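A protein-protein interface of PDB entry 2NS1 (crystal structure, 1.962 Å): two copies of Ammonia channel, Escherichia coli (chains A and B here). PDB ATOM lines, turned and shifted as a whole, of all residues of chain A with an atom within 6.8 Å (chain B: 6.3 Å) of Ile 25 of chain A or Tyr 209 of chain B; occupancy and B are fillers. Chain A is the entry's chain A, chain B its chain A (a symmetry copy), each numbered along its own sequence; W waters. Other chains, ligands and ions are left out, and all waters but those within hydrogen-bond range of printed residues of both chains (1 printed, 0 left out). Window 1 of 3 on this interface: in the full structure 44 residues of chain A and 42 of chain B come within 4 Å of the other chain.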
ATOM      1  N   ALA A  18       1.597  25.417  26.327  1.00  0.00           N
ATOM      2  CA  ALA A  18       2.619  24.707  25.513  1.00  0.00           C
ATOM      3  C   ALA A  18       3.409  25.683  24.634  1.00  0.00           C
ATOM      4  O   ALA A  18       4.632  25.577  24.484  1.00  0.00           O
ATOM      5  CB  ALA A  18       1.927  23.624  24.656  1.00  0.00           C
ATOM      6  N   VAL A  20       3.868  28.942  25.182  1.00  0.00           N
ATOM      7  CA  VAL A  20       4.800  29.750  26.004  1.00  0.00           C
ATOM      8  C   VAL A  20       6.027  28.929  26.448  1.00  0.00           C
ATOM      9  O   VAL A  20       7.161  29.429  26.489  1.00  0.00           O
ATOM     10  CB  VAL A  20       4.110  30.407  27.239  1.00  0.00           C
ATOM     11  CG1 VAL A  20       5.119  31.270  28.032  1.00  0.00           C
ATOM     12  CG2 VAL A  20       2.937  31.360  26.807  1.00  0.00           C
ATOM     13  N   LEU A  21       5.800  27.684  26.827  1.00  0.00           N
ATOM     14  CA  LEU A  21       6.908  26.791  27.196  1.00  0.00           C
ATOM     15  C   LEU A  21       7.885  26.634  26.031  1.00  0.00           C
ATOM     16  O   LEU A  21       9.094  26.601  26.228  1.00  0.00           O
ATOM     17  CB  LEU A  21       6.368  25.427  27.616  1.00  0.00           C
ATOM     18  CG  LEU A  21       5.592  25.419  28.962  1.00  0.00           C
ATOM     19  CD1 LEU A  21       4.950  24.077  29.213  1.00  0.00           C
ATOM     20  CD2 LEU A  21       6.530  25.869  30.163  1.00  0.00           C
ATOM     21  N   PHE A  22       7.344  26.567  24.822  1.00  0.00           N
ATOM     22  CA  PHE A  22       8.129  26.474  23.573  1.00  0.00           C
ATOM     23  C   PHE A  22       9.040  27.698  23.418  1.00  0.00           C
ATOM     24  O   PHE A  22      10.113  27.617  22.840  1.00  0.00           O
ATOM     25  CB  PHE A  22       7.095  26.379  22.438  1.00  0.00           C
ATOM     26  CG  PHE A  22       7.619  25.996  21.067  1.00  0.00           C
ATOM     27  CD1 PHE A  22       8.607  25.060  20.876  1.00  0.00           C
ATOM     28  CD2 PHE A  22       7.011  26.540  19.956  1.00  0.00           C
ATOM     29  CE1 PHE A  22       9.012  24.712  19.607  1.00  0.00           C
ATOM     30  CE2 PHE A  22       7.429  26.200  18.670  1.00  0.00           C
ATOM     31  CZ  PHE A  22       8.408  25.269  18.510  1.00  0.00           C
ATOM     32  N   MET A  23       8.600  28.853  23.917  1.00  0.00           N
ATOM     33  CA  MET A  23       9.413  30.049  23.833  1.00  0.00           C
ATOM     34  C   MET A  23      10.722  29.885  24.578  1.00  0.00           C
ATOM     35  O   MET A  23      11.729  30.458  24.184  1.00  0.00           O
ATOM     36  CB  MET A  23       8.673  31.279  24.405  1.00  0.00           C
ATOM     37  CG  MET A  23       7.442  31.717  23.653  1.00  0.00           C
ATOM     38  SD  MET A  23       6.544  33.010  24.580  1.00  0.00           S
ATOM     39  CE  MET A  23       7.672  34.389  24.408  1.00  0.00           C
ATOM     40  N   THR A  24      10.705  29.134  25.681  1.00  0.00           N
ATOM     41  CA  THR A  24      11.951  28.914  26.436  1.00  0.00           C
ATOM     42  C   THR A  24      12.721  27.695  25.876  1.00  0.00           C
ATOM     43  O   THR A  24      13.946  27.751  25.630  1.00  0.00           O
ATOM     44  CB  THR A  24      11.651  28.718  27.945  1.00  0.00           C
ATOM     45  OG1 THR A  24      10.912  29.834  28.439  1.00  0.00           O
ATOM     46  CG2 THR A  24      12.932  28.578  28.767  1.00  0.00           C
ATOM     47  N   ILE A  25      11.972  26.600  25.718  1.00  0.00           N
ATOM     48  CA  ILE A  25      12.459  25.282  25.325  1.00  0.00           C
ATOM     49  C   ILE A  25      11.860  25.017  23.937  1.00  0.00           C
ATOM     50  O   ILE A  25      10.759  24.520  23.807  1.00  0.00           O
ATOM     51  CB  ILE A  25      12.015  24.206  26.362  1.00  0.00           C
ATOM     52  CG1 ILE A  25      12.500  24.574  27.772  1.00  0.00           C
ATOM     53  CG2 ILE A  25      12.530  22.803  26.043  1.00  0.00           C
ATOM     54  CD1 ILE A  25      13.992  24.754  27.916  1.00  0.00           C
ATOM     55  N   PRO A  26      12.608  25.319  22.883  1.00  0.00           N
ATOM     56  CA  PRO A  26      13.971  25.783  22.807  1.00  0.00           C
ATOM     57  C   PRO A  26      14.212  27.239  22.402  1.00  0.00           C
ATOM     58  O   PRO A  26      15.353  27.600  22.218  1.00  0.00           O
ATOM     59  CB  PRO A  26      14.518  24.888  21.691  1.00  0.00           C
ATOM     60  CG  PRO A  26      13.392  24.887  20.721  1.00  0.00           C
ATOM     61  CD  PRO A  26      12.128  24.913  21.548  1.00  0.00           C
ATOM     62  N   GLY A  27      13.168  28.056  22.245  1.00  0.00           N
ATOM     63  CA  GLY A  27      13.297  29.341  21.555  1.00  0.00           C
ATOM     64  C   GLY A  27      14.427  30.218  22.044  1.00  0.00           C
ATOM     65  O   GLY A  27      15.289  30.604  21.275  1.00  0.00           O
ATOM     66  N   ILE A  28      14.410  30.563  23.325  1.00  0.00           N
ATOM     67  CA  ILE A  28      15.359  31.550  23.840  1.00  0.00           C
ATOM     68  C   ILE A  28      16.757  30.949  23.920  1.00  0.00           C
ATOM     69  O   ILE A  28      17.766  31.650  23.755  1.00  0.00           O
ATOM     70  CB  ILE A  28      14.910  32.121  25.235  1.00  0.00           C
ATOM     71  CG1 ILE A  28      15.652  33.433  25.544  1.00  0.00           C
ATOM     72  CG2 ILE A  28      15.147  31.081  26.339  1.00  0.00           C
ATOM     73  CD1 ILE A  28      15.441  34.561  24.461  1.00  0.00           C
ATOM     74  N   ALA A  29      16.818  29.643  24.146  1.00  0.00           N
ATOM     75  CA  ALA A  29      18.091  28.916  24.153  1.00  0.00           C
ATOM     76  C   ALA A  29      18.801  28.990  22.809  1.00  0.00           C
ATOM     77  O   ALA A  29      19.977  29.264  22.750  1.00  0.00           O
ATOM     78  CB  ALA A  29      17.847  27.442  24.587  1.00  0.00           C
ATOM     79  N   LEU A  45      22.618  26.635  26.396  1.00  0.00           N
ATOM     80  CA  LEU A  45      21.540  25.631  26.347  1.00  0.00           C
ATOM     81  C   LEU A  45      21.279  24.971  27.698  1.00  0.00           C
ATOM     82  O   LEU A  45      20.138  24.785  28.085  1.00  0.00           O
ATOM     83  CB  LEU A  45      21.813  24.566  25.295  1.00  0.00           C
ATOM     84  CG  LEU A  45      22.149  25.045  23.875  1.00  0.00           C
ATOM     85  CD1 LEU A  45      22.271  23.905  22.886  1.00  0.00           C
ATOM     86  CD2 LEU A  45      21.115  26.062  23.378  1.00  0.00           C
ATOM     87  N   VAL A  48      19.720  27.591  30.239  1.00  0.00           N
ATOM     88  CA  VAL A  48      18.252  27.716  29.996  1.00  0.00           C
ATOM     89  C   VAL A  48      17.511  26.470  30.459  1.00  0.00           C
ATOM     90  O   VAL A  48      16.466  26.546  31.133  1.00  0.00           O
ATOM     91  CB  VAL A  48      17.967  27.999  28.531  1.00  0.00           C
ATOM     92  CG1 VAL A  48      16.446  27.931  28.235  1.00  0.00           C
ATOM     93  CG2 VAL A  48      18.504  29.365  28.180  1.00  0.00           C
ATOM     94  N   THR A  49      18.032  25.306  30.111  1.00  0.00           N
ATOM     95  CA  THR A  49      17.302  24.057  30.423  1.00  0.00           C
ATOM     96  C   THR A  49      17.206  23.805  31.922  1.00  0.00           C
ATOM     97  O   THR A  49      16.161  23.379  32.419  1.00  0.00           O
ATOM     98  CB  THR A  49      17.948  22.826  29.767  1.00  0.00           C
ATOM     99  OG1 THR A  49      18.068  23.046  28.342  1.00  0.00           O
ATOM    100  CG2 THR A  49      17.120  21.572  30.044  1.00  0.00           C
ATOM    101  N   VAL A  50      18.307  24.004  32.635  1.00  0.00           N
ATOM    102  CA  VAL A  50      18.318  23.703  34.064  1.00  0.00           C
ATOM    103  C   VAL A  50      17.644  24.813  34.892  1.00  0.00           C
ATOM    104  O   VAL A  50      16.941  24.514  35.853  1.00  0.00           O
ATOM    105  CB  VAL A  50      19.718  23.344  34.565  1.00  0.00           C
ATOM    106  CG1 VAL A  50      19.687  23.080  36.120  1.00  0.00           C
ATOM    107  CG2 VAL A  50      20.247  22.091  33.825  1.00  0.00           C
ATOM    108  N   PHE A  52      15.148  26.518  33.708  1.00  0.00           N
ATOM    109  CA  PHE A  52      13.771  26.196  33.394  1.00  0.00           C
ATOM    110  C   PHE A  52      13.221  25.169  34.399  1.00  0.00           C
ATOM    111  O   PHE A  52      12.183  25.380  34.987  1.00  0.00           O
ATOM    112  CB  PHE A  52      13.696  25.675  31.952  1.00  0.00           C
ATOM    113  CG  PHE A  52      12.354  25.150  31.540  1.00  0.00           C
ATOM    114  CD1 PHE A  52      11.371  26.008  31.053  1.00  0.00           C
ATOM    115  CD2 PHE A  52      12.093  23.802  31.558  1.00  0.00           C
ATOM    116  CE1 PHE A  52      10.144  25.512  30.623  1.00  0.00           C
ATOM    117  CE2 PHE A  52      10.877  23.305  31.150  1.00  0.00           C
ATOM    118  CZ  PHE A  52       9.898  24.161  30.683  1.00  0.00           C
ATOM    119  N   ALA A  53      13.944  24.073  34.596  1.00  0.00           N
ATOM    120  CA  ALA A  53      13.520  22.986  35.477  1.00  0.00           C
ATOM    121  C   ALA A  53      13.381  23.483  36.916  1.00  0.00           C
ATOM    122  O   ALA A  53      12.422  23.187  37.598  1.00  0.00           O
ATOM    123  CB  ALA A  53      14.546  21.851  35.413  1.00  0.00           C
ATOM    124  N   CYS A  56      10.358  25.691  37.218  1.00  0.00           N
ATOM    125  CA  CYS A  56       9.130  24.881  37.227  1.00  0.00           C
ATOM    126  C   CYS A  56       8.856  24.285  38.600  1.00  0.00           C
ATOM    127  O   CYS A  56       7.705  24.209  39.036  1.00  0.00           O
ATOM    128  CB  CYS A  56       9.165  23.719  36.230  1.00  0.00           C
ATOM    129  SG  CYS A  56       9.112  24.192  34.464  1.00  0.00           S
ATOM    130  N   ILE A 110      10.100  31.809  31.009  1.00  0.00           N
ATOM    131  CA  ILE A 110      10.661  32.607  29.943  1.00  0.00           C
ATOM    132  C   ILE A 110      11.357  33.826  30.549  1.00  0.00           C
ATOM    133  O   ILE A 110      12.406  34.226  30.080  1.00  0.00           O
ATOM    134  CB  ILE A 110       9.620  32.929  28.798  1.00  0.00           C
ATOM    135  CG1 ILE A 110      10.258  33.723  27.659  1.00  0.00           C
ATOM    136  CG2 ILE A 110       8.362  33.638  29.344  1.00  0.00           C
ATOM    137  CD1 ILE A 110      11.481  32.995  26.941  1.00  0.00           C
ATOM    138  N   ILE A 207      10.686  30.655  16.710  1.00  0.00           N
ATOM    139  CA  ILE A 207      10.007  29.920  17.771  1.00  0.00           C
ATOM    140  C   ILE A 207       9.488  30.845  18.864  1.00  0.00           C
ATOM    141  O   ILE A 207       8.386  30.646  19.347  1.00  0.00           O
ATOM    142  CB  ILE A 207      10.906  28.778  18.336  1.00  0.00           C
ATOM    143  CG1 ILE A 207      11.138  27.761  17.225  1.00  0.00           C
ATOM    144  CG2 ILE A 207      10.272  28.165  19.664  1.00  0.00           C
ATOM    145  CD1 ILE A 207      12.108  26.607  17.523  1.00  0.00           C
ATOM    146  N   MET B  23       6.383  15.350  17.560  1.00  0.00           N
ATOM    147  CA  MET B  23       7.359  14.596  18.320  1.00  0.00           C
ATOM    148  C   MET B  23       8.193  13.702  17.424  1.00  0.00           C
ATOM    149  O   MET B  23       9.357  13.461  17.710  1.00  0.00           O
ATOM    150  CB  MET B  23       6.684  13.720  19.399  1.00  0.00           C
ATOM    151  CG  MET B  23       5.973  14.461  20.501  1.00  0.00           C
ATOM    152  SD  MET B  23       5.022  13.304  21.548  1.00  0.00           S
ATOM    153  CE  MET B  23       6.349  12.445  22.387  1.00  0.00           C
ATOM    154  N   PHE B 202      19.580  18.918  21.512  1.00  0.00           N
ATOM    155  CA  PHE B 202      18.765  19.805  22.333  1.00  0.00           C
ATOM    156  C   PHE B 202      17.471  20.243  21.640  1.00  0.00           C
ATOM    157  O   PHE B 202      16.412  20.246  22.246  1.00  0.00           O
ATOM    158  CB  PHE B 202      19.567  21.029  22.772  1.00  0.00           C
ATOM    159  CG  PHE B 202      18.719  22.099  23.384  1.00  0.00           C
ATOM    160  CD1 PHE B 202      18.311  22.006  24.705  1.00  0.00           C
ATOM    161  CD2 PHE B 202      18.303  23.191  22.636  1.00  0.00           C
ATOM    162  CE1 PHE B 202      17.510  22.960  25.260  1.00  0.00           C
ATOM    163  CE2 PHE B 202      17.497  24.156  23.204  1.00  0.00           C
ATOM    164  CZ  PHE B 202      17.126  24.061  24.525  1.00  0.00           C
ATOM    165  N   GLY B 204      15.865  18.641  19.264  1.00  0.00           N
ATOM    166  CA  GLY B 204      14.999  17.474  19.268  1.00  0.00           C
ATOM    167  C   GLY B 204      14.352  17.221  20.617  1.00  0.00           C
ATOM    168  O   GLY B 204      13.175  16.857  20.674  1.00  0.00           O
ATOM    169  N   THR B 205      15.110  17.422  21.687  1.00  0.00           N
ATOM    170  CA  THR B 205      14.631  17.235  23.056  1.00  0.00           C
ATOM    171  C   THR B 205      13.495  18.191  23.323  1.00  0.00           C
ATOM    172  O   THR B 205      12.474  17.817  23.887  1.00  0.00           O
ATOM    173  CB  THR B 205      15.743  17.514  24.122  1.00  0.00           C
ATOM    174  OG1 THR B 205      16.865  16.656  23.880  1.00  0.00           O
ATOM    175  CG2 THR B 205      15.210  17.295  25.546  1.00  0.00           C
ATOM    176  N   ALA B 206      13.689  19.434  22.904  1.00  0.00           N
ATOM    177  CA  ALA B 206      12.745  20.498  23.149  1.00  0.00           C
ATOM    178  C   ALA B 206      11.437  20.228  22.450  1.00  0.00           C
ATOM    179  O   ALA B 206      10.366  20.378  23.033  1.00  0.00           O
ATOM    180  CB  ALA B 206      13.338  21.817  22.672  1.00  0.00           C
ATOM    181  N   ILE B 207      11.537  19.791  21.199  1.00  0.00           N
ATOM    182  CA  ILE B 207      10.361  19.475  20.397  1.00  0.00           C
ATOM    183  C   ILE B 207       9.614  18.260  20.932  1.00  0.00           C
ATOM    184  O   ILE B 207       8.395  18.269  20.962  1.00  0.00           O
ATOM    185  CB  ILE B 207      10.726  19.329  18.887  1.00  0.00           C
ATOM    186  CG1 ILE B 207      11.207  20.685  18.382  1.00  0.00           C
ATOM    187  CG2 ILE B 207       9.503  18.721  18.067  1.00  0.00           C
ATOM    188  CD1 ILE B 207      11.743  20.746  16.943  1.00  0.00           C
ATOM    189  N   LEU B 208      10.347  17.224  21.345  1.00  0.00           N
ATOM    190  CA  LEU B 208       9.763  16.075  22.033  1.00  0.00           C
ATOM    191  C   LEU B 208       9.009  16.525  23.269  1.00  0.00           C
ATOM    192  O   LEU B 208       7.912  16.055  23.527  1.00  0.00           O
ATOM    193  CB  LEU B 208      10.841  15.042  22.441  1.00  0.00           C
ATOM    194  CG  LEU B 208      11.408  14.153  21.331  1.00  0.00           C
ATOM    195  CD1 LEU B 208      12.775  13.508  21.736  1.00  0.00           C
ATOM    196  CD2 LEU B 208      10.392  13.105  20.948  1.00  0.00           C
ATOM    197  N   TYR B 209       9.619  17.406  24.056  1.00  0.00           N
ATOM    198  CA  TYR B 209       8.987  17.917  25.283  1.00  0.00           C
ATOM    199  C   TYR B 209       7.682  18.656  24.962  1.00  0.00           C
ATOM    200  O   TYR B 209       6.621  18.366  25.538  1.00  0.00           O
ATOM    201  CB  TYR B 209       9.959  18.827  26.035  1.00  0.00           C
ATOM    202  CG  TYR B 209       9.365  19.602  27.201  1.00  0.00           C
ATOM    203  CD1 TYR B 209       8.971  18.957  28.379  1.00  0.00           C
ATOM    204  CD2 TYR B 209       9.195  20.983  27.134  1.00  0.00           C
ATOM    205  CE1 TYR B 209       8.438  19.672  29.452  1.00  0.00           C
ATOM    206  CE2 TYR B 209       8.674  21.689  28.200  1.00  0.00           C
ATOM    207  CZ  TYR B 209       8.307  21.029  29.368  1.00  0.00           C
ATOM    208  OH  TYR B 209       7.758  21.747  30.420  1.00  0.00           O
ATOM    209  N   ILE B 210       7.737  19.582  24.006  1.00  0.00           N
ATOM    210  CA  ILE B 210       6.556  20.375  23.690  1.00  0.00           C
ATOM    211  C   ILE B 210       5.438  19.489  23.103  1.00  0.00           C
ATOM    212  O   ILE B 210       4.282  19.598  23.493  1.00  0.00           O
ATOM    213  CB  ILE B 210       6.884  21.574  22.762  1.00  0.00           C
ATOM    214  CG1 ILE B 210       7.833  22.575  23.479  1.00  0.00           C
ATOM    215  CG2 ILE B 210       5.567  22.265  22.298  1.00  0.00           C
ATOM    216  CD1 ILE B 210       7.359  23.099  24.839  1.00  0.00           C
ATOM    217  N   GLY B 211       5.787  18.581  22.202  1.00  0.00           N
ATOM    218  CA  GLY B 211       4.802  17.677  21.640  1.00  0.00           C
ATOM    219  C   GLY B 211       4.195  16.732  22.654  1.00  0.00           C
ATOM    220  O   GLY B 211       3.050  16.299  22.514  1.00  0.00           O
ATOM    221  N   TRP B 212       4.970  16.426  23.690  1.00  0.00           N
ATOM    222  CA  TRP B 212       4.546  15.511  24.747  1.00  0.00           C
ATOM    223  C   TRP B 212       3.334  16.005  25.501  1.00  0.00           C
ATOM    224  O   TRP B 212       2.610  15.217  26.094  1.00  0.00           O
ATOM    225  CB  TRP B 212       5.716  15.249  25.698  1.00  0.00           C
ATOM    226  CG  TRP B 212       5.811  13.821  26.140  1.00  0.00           C
ATOM    227  CD1 TRP B 212       4.896  13.149  26.876  1.00  0.00           C
ATOM    228  CD2 TRP B 212       6.904  12.930  25.951  1.00  0.00           C
ATOM    229  NE1 TRP B 212       5.345  11.885  27.149  1.00  0.00           N
ATOM    230  CE2 TRP B 212       6.575  11.723  26.591  1.00  0.00           C
ATOM    231  CE3 TRP B 212       8.141  13.034  25.317  1.00  0.00           C
ATOM    232  CZ2 TRP B 212       7.442  10.622  26.613  1.00  0.00           C
ATOM    233  CZ3 TRP B 212       8.984  11.944  25.317  1.00  0.00           C
ATOM    234  CH2 TRP B 212       8.632  10.754  25.961  1.00  0.00           C
ATOM    235  N   PHE B 213       3.079  17.316  25.485  1.00  0.00           N
ATOM    236  CA  PHE B 213       1.855  17.819  26.113  1.00  0.00           C
ATOM    237  C   PHE B 213       0.670  17.325  25.350  1.00  0.00           C
ATOM    238  O   PHE B 213      -0.331  16.961  25.941  1.00  0.00           O
ATOM    239  CB  PHE B 213       1.856  19.339  26.263  1.00  0.00           C
ATOM    240  CG  PHE B 213       2.849  19.783  27.262  1.00  0.00           C
ATOM    241  CD1 PHE B 213       2.587  19.623  28.604  1.00  0.00           C
ATOM    242  CD2 PHE B 213       4.094  20.211  26.875  1.00  0.00           C
ATOM    243  CE1 PHE B 213       3.515  19.971  29.545  1.00  0.00           C
ATOM    244  CE2 PHE B 213       5.053  20.561  27.832  1.00  0.00           C
ATOM    245  CZ  PHE B 213       4.751  20.436  29.158  1.00  0.00           C
ATOM    246  N   GLY B 214       0.777  17.282  24.030  1.00  0.00           N
ATOM    247  CA  GLY B 214      -0.258  16.660  23.225  1.00  0.00           C
ATOM    248  C   GLY B 214      -0.476  15.177  23.538  1.00  0.00           C
ATOM    249  O   GLY B 214      -1.621  14.689  23.586  1.00  0.00           O
ATOM    250  N   THR B 234       3.094  16.598  33.765  1.00  0.00           N
ATOM    251  CA  THR B 234       4.125  16.549  32.740  1.00  0.00           C
ATOM    252  C   THR B 234       5.185  17.649  32.991  1.00  0.00           C
ATOM    253  O   THR B 234       6.372  17.391  32.943  1.00  0.00           O
ATOM    254  CB  THR B 234       3.493  16.646  31.353  1.00  0.00           C
ATOM    255  OG1 THR B 234       2.579  15.539  31.188  1.00  0.00           O
ATOM    256  CG2 THR B 234       4.571  16.616  30.247  1.00  0.00           C
ATOM    257  N   VAL B 235       4.755  18.852  33.296  1.00  0.00           N
ATOM    258  CA  VAL B 235       5.691  19.925  33.603  1.00  0.00           C
ATOM    259  C   VAL B 235       6.570  19.511  34.781  1.00  0.00           C
ATOM    260  O   VAL B 235       7.811  19.600  34.731  1.00  0.00           O
ATOM    261  CB  VAL B 235       4.955  21.240  33.900  1.00  0.00           C
ATOM    262  CG1 VAL B 235       5.930  22.301  34.401  1.00  0.00           C
ATOM    263  CG2 VAL B 235       4.242  21.769  32.627  1.00  0.00           C
ATOM    264  N   THR B 238       8.967  16.318  34.370  1.00  0.00           N
ATOM    265  CA  THR B 238      10.109  16.595  33.474  1.00  0.00           C
ATOM    266  C   THR B 238      11.165  17.430  34.203  1.00  0.00           C
ATOM    267  O   THR B 238      12.356  17.135  34.156  1.00  0.00           O
ATOM    268  CB  THR B 238       9.642  17.360  32.223  1.00  0.00           C
ATOM    269  OG1 THR B 238       8.620  16.603  31.575  1.00  0.00           O
ATOM    270  CG2 THR B 238      10.811  17.600  31.255  1.00  0.00           C
ATOM    271  N   ALA B 239      10.710  18.496  34.854  1.00  0.00           N
ATOM    272  CA  ALA B 239      11.604  19.414  35.584  1.00  0.00           C
ATOM    273  C   ALA B 239      12.349  18.647  36.697  1.00  0.00           C
ATOM    274  O   ALA B 239      13.551  18.819  36.893  1.00  0.00           O
ATOM    275  CB  ALA B 239      10.763  20.568  36.189  1.00  0.00           C
ATOM    276  N   ALA B 265      15.265  15.183  30.989  1.00  0.00           N
ATOM    277  CA  ALA B 265      13.956  15.608  30.511  1.00  0.00           C
ATOM    278  C   ALA B 265      13.186  14.429  29.960  1.00  0.00           C
ATOM    279  O   ALA B 265      12.034  14.177  30.343  1.00  0.00           O
ATOM    280  CB  ALA B 265      14.146  16.693  29.396  1.00  0.00           C
ATOM    281  N   ILE B 266      13.828  13.687  29.056  1.00  0.00           N
ATOM    282  CA  ILE B 266      13.199  12.527  28.431  1.00  0.00           C
ATOM    283  C   ILE B 266      12.835  11.459  29.471  1.00  0.00           C
ATOM    284  O   ILE B 266      11.769  10.889  29.411  1.00  0.00           O
ATOM    285  CB  ILE B 266      14.056  11.907  27.298  1.00  0.00           C
ATOM    286  CG1 ILE B 266      14.410  12.965  26.221  1.00  0.00           C
ATOM    287  CG2 ILE B 266      13.306  10.751  26.629  1.00  0.00           C
ATOM    288  CD1 ILE B 266      13.179  13.706  25.652  1.00  0.00           C
ATOM    289  N   LEU B 269       9.684  12.543  31.232  1.00  0.00           N
ATOM    290  CA  LEU B 269       8.551  12.436  30.329  1.00  0.00           C
ATOM    291  C   LEU B 269       8.113  10.987  30.170  1.00  0.00           C
ATOM    292  O   LEU B 269       6.922  10.658  30.178  1.00  0.00           O
ATOM    293  CB  LEU B 269       8.961  12.987  28.960  1.00  0.00           C
ATOM    294  CG  LEU B 269       9.060  14.512  28.978  1.00  0.00           C
ATOM    295  CD1 LEU B 269       9.867  15.000  27.773  1.00  0.00           C
ATOM    296  CD2 LEU B 269       7.619  15.107  29.030  1.00  0.00           C
HETATM  297  O   HOH W   1       8.992  21.174  32.790  1.00  0.00           O
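The backbone carbonyl oxygen (O) of Phe 22 of chain A lies within hydrogen-bond range of the backbone NH (N) of Gly 27 of chain A (3.1 Å).
O of Phe 52 of chain A lies within hydrogen-bond range of SG of Cys 56 of chain A, 3.3 Å away.
The side-chain hydroxyl (OG1) of Thr 49 of chain A is in hydrogen-bond range of the backbone carbonyl oxygen (O) of Leu 45 of chain A, 2.7 Å away.
CD1 of Leu 21 of chain A touches OH of Tyr 209 of chain B (3.8 Å).
Ile 210 of chain B touches Leu 21 of chain A.
CD1 of Leu 21 of chain A touches CZ of Phe 213 of chain B, at 3.6 Å.
N of Phe 22 of chain A touches CD1 of Ile 210 of chain B, at 3.5 Å.
Ile 25 of chain A touches Tyr 209 of chain B.
CE2 of Phe 202 of chain B touches CB of Pro 26 of chain A, at 3.4 Å.
Ala 29 of chain A touches Phe 202 of chain B (CB to CZ, 3.5 Å).
Leu 45 of chain A touches Phe 202 of chain B.
Thr 49 of chain A touches Phe 202 of chain B.
Cys 56 of chain A touches Ala 239 of chain B.
Of the printed residues of chain B, Leu 21 of chain A touches Tyr 209, Ile 210 and Phe 213.
Ile 25 of chain A touches just these residues of chain B: Ala 206, Tyr 209 and Ile 210.
Of the printed residues of chain B, Leu 45 of chain A touches Phe 202 (3.9 Å).
Of the printed residues of chain B, Phe 52 of chain A touches Tyr 209 (3.2 Å).
Printed residues of chain B within 4 Å of Cys 56 of chain A: Val 235 (3.7 Å) and Ala 239 (3.5 Å).
Of chain A, only Leu 21, Ile 25 and Phe 52 come within 4 Å of Tyr 209 of chain B.
Of the printed residues of chain A, Phe 213 of chain B touches Leu 21.
Thr 238 of chain B touches none of the printed residues of chain A.
The nearest residue of chain B that does not touch Ile 25 of chain A is Phe 202 of chain B (4.7 Å).
The nearest residue of chain A that does not touch Tyr 209 of chain B is Cys 56 of chain A (4.9 Å).
Of the 20 printed residues of chain B, 7 touch a printed residue of chain A.
Hydrophobic or aromatic side chains of chain B that line the printed part of chain A: Phe 202, Ala 206, Tyr 209, Ile 210, Phe 213, Val 235 and Ala 239.
Along chain B the printed residues that touch a printed residue of chain A span positions 202 to 239.
Of the 20 printed residues of chain A, 11 touch a printed residue of chain B.
Hydrophobic or aromatic side chains of chain A within 4 Å of the printed part of chain B: Leu 21, Phe 22, Ile 25, Pro 26, Ala 29, Leu 45, Phe 52 and Ala 53.
Positions printed for both chains: 23 and 207.
Water W1 lies within hydrogen-bond range of the side-chain hydroxyl of Tyr 209 of chain B, the backbone carbonyl oxygen of Val 235 of chain B and the side-chain sulfur of Cys 56 of chain A.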
